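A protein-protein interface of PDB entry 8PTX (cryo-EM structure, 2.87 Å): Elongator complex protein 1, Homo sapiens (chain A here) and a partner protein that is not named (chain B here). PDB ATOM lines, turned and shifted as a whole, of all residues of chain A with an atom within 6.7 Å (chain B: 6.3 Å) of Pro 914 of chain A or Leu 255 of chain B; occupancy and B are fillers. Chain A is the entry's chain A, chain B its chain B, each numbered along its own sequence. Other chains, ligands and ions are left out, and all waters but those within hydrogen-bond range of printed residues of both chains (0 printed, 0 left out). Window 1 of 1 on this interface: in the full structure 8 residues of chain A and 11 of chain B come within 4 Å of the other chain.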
ATOM      1  N   LEU A 904     -31.463 -11.104   3.873  1.00  0.00           N
ATOM      2  CA  LEU A 904     -31.928 -10.055   4.775  1.00  0.00           C
ATOM      3  C   LEU A 904     -33.350 -10.324   5.244  1.00  0.00           C
ATOM      4  O   LEU A 904     -33.672 -10.126   6.424  1.00  0.00           O
ATOM      5  CB  LEU A 904     -31.836  -8.696   4.087  1.00  0.00           C
ATOM      6  CG  LEU A 904     -30.455  -8.047   4.081  1.00  0.00           C
ATOM      7  CD1 LEU A 904     -30.392  -6.960   3.026  1.00  0.00           C
ATOM      8  CD2 LEU A 904     -30.123  -7.487   5.452  1.00  0.00           C
ATOM      9  N   ALA A 907     -33.091 -13.008   7.880  1.00  0.00           N
ATOM     10  CA  ALA A 907     -32.368 -12.555   9.059  1.00  0.00           C
ATOM     11  C   ALA A 907     -33.135 -11.506   9.847  1.00  0.00           C
ATOM     12  O   ALA A 907     -32.811 -11.275  11.017  1.00  0.00           O
ATOM     13  CB  ALA A 907     -31.002 -12.002   8.655  1.00  0.00           C
ATOM     14  N   GLU A 908     -34.126 -10.855   9.234  1.00  0.00           N
ATOM     15  CA  GLU A 908     -34.951  -9.909   9.981  1.00  0.00           C
ATOM     16  C   GLU A 908     -35.596 -10.578  11.188  1.00  0.00           C
ATOM     17  O   GLU A 908     -35.493 -10.085  12.316  1.00  0.00           O
ATOM     18  CB  GLU A 908     -36.020  -9.310   9.069  1.00  0.00           C
ATOM     19  CG  GLU A 908     -35.535  -8.160   8.209  1.00  0.00           C
ATOM     20  CD  GLU A 908     -36.065  -8.237   6.793  1.00  0.00           C
ATOM     21  OE1 GLU A 908     -37.125  -8.865   6.590  1.00  0.00           O
ATOM     22  OE2 GLU A 908     -35.424  -7.670   5.885  1.00  0.00           O
ATOM     23  N   LYS A 912     -30.829 -11.883  15.982  1.00  0.00           N
ATOM     24  CA  LYS A 912     -29.385 -11.814  15.838  1.00  0.00           C
ATOM     25  C   LYS A 912     -28.928 -10.363  15.855  1.00  0.00           C
ATOM     26  O   LYS A 912     -29.693  -9.449  15.540  1.00  0.00           O
ATOM     27  CB  LYS A 912     -28.908 -12.482  14.542  1.00  0.00           C
ATOM     28  CG  LYS A 912     -29.038 -13.990  14.538  1.00  0.00           C
ATOM     29  CD  LYS A 912     -28.410 -14.593  13.297  1.00  0.00           C
ATOM     30  CE  LYS A 912     -28.497 -16.105  13.331  1.00  0.00           C
ATOM     31  NZ  LYS A 912     -27.807 -16.727  12.177  1.00  0.00           N
ATOM     32  N   ASP A 913     -27.672 -10.167  16.224  1.00  0.00           N
ATOM     33  CA  ASP A 913     -27.086  -8.834  16.259  1.00  0.00           C
ATOM     34  C   ASP A 913     -26.793  -8.366  14.838  1.00  0.00           C
ATOM     35  O   ASP A 913     -26.039  -9.035  14.121  1.00  0.00           O
ATOM     36  CB  ASP A 913     -25.809  -8.859  17.093  1.00  0.00           C
ATOM     37  CG  ASP A 913     -25.292  -7.477  17.423  1.00  0.00           C
ATOM     38  OD1 ASP A 913     -25.801  -6.491  16.855  1.00  0.00           O
ATOM     39  OD2 ASP A 913     -24.371  -7.376  18.257  1.00  0.00           O
ATOM     40  N   PRO A 914     -27.369  -7.247  14.384  1.00  0.00           N
ATOM     41  CA  PRO A 914     -27.046  -6.767  13.031  1.00  0.00           C
ATOM     42  C   PRO A 914     -25.576  -6.447  12.845  1.00  0.00           C
ATOM     43  O   PRO A 914     -25.025  -6.684  11.761  1.00  0.00           O
ATOM     44  CB  PRO A 914     -27.924  -5.516  12.883  1.00  0.00           C
ATOM     45  CG  PRO A 914     -28.266  -5.121  14.267  1.00  0.00           C
ATOM     46  CD  PRO A 914     -28.358  -6.388  15.050  1.00  0.00           C
ATOM     47  N   LYS A 915     -24.919  -5.909  13.874  1.00  0.00           N
ATOM     48  CA  LYS A 915     -23.487  -5.647  13.788  1.00  0.00           C
ATOM     49  C   LYS A 915     -22.659  -6.882  14.098  1.00  0.00           C
ATOM     50  O   LYS A 915     -21.691  -6.821  14.859  1.00  0.00           O
ATOM     51  CB  LYS A 915     -23.129  -4.505  14.736  1.00  0.00           C
ATOM     52  CG  LYS A 915     -24.075  -3.321  14.663  1.00  0.00           C
ATOM     53  CD  LYS A 915     -23.335  -2.013  14.868  1.00  0.00           C
ATOM     54  CE  LYS A 915     -24.087  -0.845  14.260  1.00  0.00           C
ATOM     55  NZ  LYS A 915     -23.283   0.406  14.316  1.00  0.00           N
ATOM     56  N   GLU A 916     -23.030  -8.017  13.512  1.00  0.00           N
ATOM     57  CA  GLU A 916     -22.223  -9.226  13.557  1.00  0.00           C
ATOM     58  C   GLU A 916     -22.242  -9.866  12.178  1.00  0.00           C
ATOM     59  O   GLU A 916     -21.292 -10.551  11.787  1.00  0.00           O
ATOM     60  CB  GLU A 916     -22.743 -10.185  14.629  1.00  0.00           C
ATOM     61  CG  GLU A 916     -21.836 -11.373  14.917  1.00  0.00           C
ATOM     62  CD  GLU A 916     -22.038 -12.517  13.945  1.00  0.00           C
ATOM     63  OE1 GLU A 916     -23.163 -12.661  13.425  1.00  0.00           O
ATOM     64  OE2 GLU A 916     -21.072 -13.268  13.695  1.00  0.00           O
ATOM     65  N   TYR A 917     -23.323  -9.634  11.430  1.00  0.00           N
ATOM     66  CA  TYR A 917     -23.467 -10.196  10.098  1.00  0.00           C
ATOM     67  C   TYR A 917     -23.602  -9.153   9.001  1.00  0.00           C
ATOM     68  O   TYR A 917     -23.459  -9.504   7.826  1.00  0.00           O
ATOM     69  CB  TYR A 917     -24.671 -11.152  10.039  1.00  0.00           C
ATOM     70  CG  TYR A 917     -26.032 -10.493  10.097  1.00  0.00           C
ATOM     71  CD1 TYR A 917     -26.656 -10.254  11.311  1.00  0.00           C
ATOM     72  CD2 TYR A 917     -26.705 -10.137   8.935  1.00  0.00           C
ATOM     73  CE1 TYR A 917     -27.904  -9.666  11.370  1.00  0.00           C
ATOM     74  CE2 TYR A 917     -27.951  -9.546   8.985  1.00  0.00           C
ATOM     75  CZ  TYR A 917     -28.545  -9.312  10.204  1.00  0.00           C
ATOM     76  OH  TYR A 917     -29.786  -8.725  10.256  1.00  0.00           O
ATOM     77  N   LEU A 918     -23.877  -7.894   9.340  1.00  0.00           N
ATOM     78  CA  LEU A 918     -23.818  -6.850   8.320  1.00  0.00           C
ATOM     79  C   LEU A 918     -22.418  -6.695   7.736  1.00  0.00           C
ATOM     80  O   LEU A 918     -22.289  -6.679   6.498  1.00  0.00           O
ATOM     81  CB  LEU A 918     -24.346  -5.532   8.896  1.00  0.00           C
ATOM     82  CG  LEU A 918     -25.853  -5.317   8.781  1.00  0.00           C
ATOM     83  CD1 LEU A 918     -26.230  -3.942   9.293  1.00  0.00           C
ATOM     84  CD2 LEU A 918     -26.305  -5.495   7.344  1.00  0.00           C
ATOM     85  N   PRO A 919     -21.344  -6.586   8.531  1.00  0.00           N
ATOM     86  CA  PRO A 919     -20.005  -6.569   7.916  1.00  0.00           C
ATOM     87  C   PRO A 919     -19.698  -7.832   7.138  1.00  0.00           C
ATOM     88  O   PRO A 919     -19.018  -7.770   6.107  1.00  0.00           O
ATOM     89  CB  PRO A 919     -19.070  -6.400   9.121  1.00  0.00           C
ATOM     90  CG  PRO A 919     -19.915  -5.805  10.181  1.00  0.00           C
ATOM     91  CD  PRO A 919     -21.260  -6.422   9.993  1.00  0.00           C
ATOM     92  N   ILE B 253     -25.227  -3.283   1.567  1.00  0.00           N
ATOM     93  CA  ILE B 253     -26.247  -4.098   2.213  1.00  0.00           C
ATOM     94  C   ILE B 253     -26.697  -3.366   3.467  1.00  0.00           C
ATOM     95  O   ILE B 253     -25.902  -3.158   4.391  1.00  0.00           O
ATOM     96  CB  ILE B 253     -25.720  -5.501   2.547  1.00  0.00           C
ATOM     97  CG1 ILE B 253     -25.307  -6.235   1.271  1.00  0.00           C
ATOM     98  CG2 ILE B 253     -26.762  -6.291   3.313  1.00  0.00           C
ATOM     99  CD1 ILE B 253     -26.297  -6.103   0.137  1.00  0.00           C
ATOM    100  N   ARG B 254     -27.968  -2.976   3.502  1.00  0.00           N
ATOM    101  CA  ARG B 254     -28.507  -2.210   4.613  1.00  0.00           C
ATOM    102  C   ARG B 254     -29.856  -2.777   5.025  1.00  0.00           C
ATOM    103  O   ARG B 254     -30.621  -3.271   4.192  1.00  0.00           O
ATOM    104  CB  ARG B 254     -28.653  -0.727   4.252  1.00  0.00           C
ATOM    105  CG  ARG B 254     -27.334   0.019   4.157  1.00  0.00           C
ATOM    106  CD  ARG B 254     -27.557   1.473   3.782  1.00  0.00           C
ATOM    107  NE  ARG B 254     -28.021   1.605   2.406  1.00  0.00           N
ATOM    108  CZ  ARG B 254     -29.225   2.037   2.058  1.00  0.00           C
ATOM    109  NH1 ARG B 254     -30.120   2.394   2.964  1.00  0.00           N
ATOM    110  NH2 ARG B 254     -29.540   2.110   0.768  1.00  0.00           N
ATOM    111  N   LEU B 255     -30.140  -2.697   6.321  1.00  0.00           N
ATOM    112  CA  LEU B 255     -31.432  -3.122   6.835  1.00  0.00           C
ATOM    113  C   LEU B 255     -32.538  -2.227   6.291  1.00  0.00           C
ATOM    114  O   LEU B 255     -32.339  -1.035   6.046  1.00  0.00           O
ATOM    115  CB  LEU B 255     -31.442  -3.085   8.361  1.00  0.00           C
ATOM    116  CG  LEU B 255     -30.495  -4.038   9.087  1.00  0.00           C
ATOM    117  CD1 LEU B 255     -30.350  -3.632  10.543  1.00  0.00           C
ATOM    118  CD2 LEU B 255     -30.995  -5.465   8.978  1.00  0.00           C
ATOM    119  N   LYS B 256     -33.712  -2.818   6.094  1.00  0.00           N
ATOM    120  CA  LYS B 256     -34.855  -2.052   5.624  1.00  0.00           C
ATOM    121  C   LYS B 256     -35.284  -1.047   6.687  1.00  0.00           C
ATOM    122  O   LYS B 256     -35.308  -1.354   7.881  1.00  0.00           O
ATOM    123  CB  LYS B 256     -36.011  -2.983   5.271  1.00  0.00           C
ATOM    124  CG  LYS B 256     -37.224  -2.270   4.708  1.00  0.00           C
ATOM    125  CD  LYS B 256     -36.883  -1.584   3.396  1.00  0.00           C
ATOM    126  CE  LYS B 256     -38.078  -0.824   2.843  1.00  0.00           C
ATOM    127  NZ  LYS B 256     -39.186  -1.741   2.454  1.00  0.00           N
ATOM    128  N   GLU B 257     -35.619   0.159   6.245  1.00  0.00           N
ATOM    129  CA  GLU B 257     -35.957   1.260   7.135  1.00  0.00           C
ATOM    130  C   GLU B 257     -37.457   1.292   7.387  1.00  0.00           C
ATOM    131  O   GLU B 257     -38.252   1.046   6.477  1.00  0.00           O
ATOM    132  CB  GLU B 257     -35.507   2.592   6.536  1.00  0.00           C
ATOM    133  CG  GLU B 257     -34.007   2.733   6.392  1.00  0.00           C
ATOM    134  CD  GLU B 257     -33.611   4.036   5.733  1.00  0.00           C
ATOM    135  OE1 GLU B 257     -34.510   4.755   5.251  1.00  0.00           O
ATOM    136  OE2 GLU B 257     -32.400   4.342   5.698  1.00  0.00           O
ATOM    137  N   THR B 274     -34.566   2.449  12.619  1.00  0.00           N
ATOM    138  CA  THR B 274     -33.807   1.250  12.292  1.00  0.00           C
ATOM    139  C   THR B 274     -33.091   0.758  13.545  1.00  0.00           C
ATOM    140  O   THR B 274     -32.639   1.549  14.375  1.00  0.00           O
ATOM    141  CB  THR B 274     -32.809   1.523  11.157  1.00  0.00           C
ATOM    142  OG1 THR B 274     -33.528   1.803   9.949  1.00  0.00           O
ATOM    143  CG2 THR B 274     -31.902   0.330  10.918  1.00  0.00           C
ATOM    144  N   LEU B 275     -33.000  -0.565  13.676  1.00  0.00           N
ATOM    145  CA  LEU B 275     -32.368  -1.193  14.827  1.00  0.00           C
ATOM    146  C   LEU B 275     -30.859  -0.982  14.773  1.00  0.00           C
ATOM    147  O   LEU B 275     -30.268  -0.916  13.694  1.00  0.00           O
ATOM    148  CB  LEU B 275     -32.699  -2.686  14.867  1.00  0.00           C
ATOM    149  CG  LEU B 275     -32.416  -3.494  16.139  1.00  0.00           C
ATOM    150  CD1 LEU B 275     -33.377  -4.661  16.223  1.00  0.00           C
ATOM    151  CD2 LEU B 275     -30.995  -4.002  16.201  1.00  0.00           C
ATOM    152  N   GLU B 276     -30.242  -0.868  15.947  1.00  0.00           N
ATOM    153  CA  GLU B 276     -28.813  -0.609  16.059  1.00  0.00           C
ATOM    154  C   GLU B 276     -28.014  -1.818  16.522  1.00  0.00           C
ATOM    155  O   GLU B 276     -27.072  -2.229  15.839  1.00  0.00           O
ATOM    156  CB  GLU B 276     -28.572   0.560  17.023  1.00  0.00           C
ATOM    157  CG  GLU B 276     -27.131   1.009  17.116  1.00  0.00           C
ATOM    158  CD  GLU B 276     -26.683   1.766  15.890  1.00  0.00           C
ATOM    159  OE1 GLU B 276     -27.552   2.313  15.183  1.00  0.00           O
ATOM    160  OE2 GLU B 276     -25.463   1.822  15.635  1.00  0.00           O
ATOM    161  N   THR B 277     -28.362  -2.403  17.665  1.00  0.00           N
ATOM    162  CA  THR B 277     -27.583  -3.495  18.234  1.00  0.00           C
ATOM    163  C   THR B 277     -28.467  -4.306  19.169  1.00  0.00           C
ATOM    164  O   THR B 277     -29.583  -3.900  19.501  1.00  0.00           O
ATOM    165  CB  THR B 277     -26.350  -2.976  18.979  1.00  0.00           C
ATOM    166  OG1 THR B 277     -25.528  -4.078  19.375  1.00  0.00           O
ATOM    167  CG2 THR B 277     -26.767  -2.207  20.210  1.00  0.00           C
ATOM    168  N   VAL B 278     -27.958  -5.465  19.581  1.00  0.00           N
ATOM    169  CA  VAL B 278     -28.651  -6.369  20.499  1.00  0.00           C
ATOM    170  C   VAL B 278     -27.622  -6.871  21.504  1.00  0.00           C
ATOM    171  O   VAL B 278     -26.782  -7.713  21.172  1.00  0.00           O
ATOM    172  CB  VAL B 278     -29.324  -7.541  19.777  1.00  0.00           C
ATOM    173  CG1 VAL B 278     -29.953  -8.480  20.782  1.00  0.00           C
ATOM    174  CG2 VAL B 278     -30.370  -7.041  18.804  1.00  0.00           C
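The side-chain carboxylate (OD1) of Asp 913 of chain A lies within hydrogen-bond range of the side-chain hydroxyl (OG1) of Thr 277 of chain B, at 3.5 Å. The side-chain amino group of Lys 915 of chain A lies within salt-bridge range of the side-chain carboxylate of Glu 276 of chain B (2.9 Å).
OD1 of Asp 913 of chain A lies within hydrogen-bond range of N of Lys 915 of chain A, at 3.2 Å.
Ile 253 of chain B touches Leu 904 of chain A. Leu 904 of chain A touches Arg 254 of chain B. Val 278 of chain B touches Asp 913 of chain A (N to OD1, 3.6 Å). CB of Pro 914 of chain A touches CD1 of Leu 255 of chain B (3.9 Å). CD2 of Leu 275 of chain B touches CG of Pro 914 of chain A, 3.5 Å away. CG of Pro 914 of chain A touches O of Glu 276 of chain B, at 3.5 Å. Tyr 917 of chain A touches Leu 255 of chain B. Leu 918 of chain A touches Ile 253 of chain B.
Glu 916 of chain A touches none of the printed residues of chain B. Of the printed residues of chain B, Tyr 917 of chain A touches Leu 255 (3.7 Å). Printed residues of chain B within 4 Å of Leu 918 of chain A: Ile 253 (3.8 Å). Printed residues of chain A within 4 Å of Ile 253 of chain B: Leu 904 and Leu 918. Leu 255 of chain B touches just these residues of chain A: Pro 914 and Tyr 917. Lys 256 of chain B touches none of the printed residues of chain A. Printed residues of chain A within 4 Å of Leu 275 of chain B: Pro 914. Printed residues of chain A within 4 Å of Thr 277 of chain B: Asp 913 (3.5 Å). The nearest residue of chain A that does not touch Leu 255 of chain B is Leu 904 of chain A (4.2 Å).
Of the 11 printed residues of chain A, 6 touch a printed residue of chain B. Of the 10 printed residues of chain B, 7 touch a printed residue of chain A. Hydrophobic or aromatic side chains of chain B within 4 Å of the printed part of chain A: Ile 253, Leu 255 and Leu 275. Among the printed residues, Asp or Glu carboxylates within 4 Å of a Lys or Arg side-chain nitrogen of the other chain: Lys 915 of chain A with Glu 276 of chain B.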
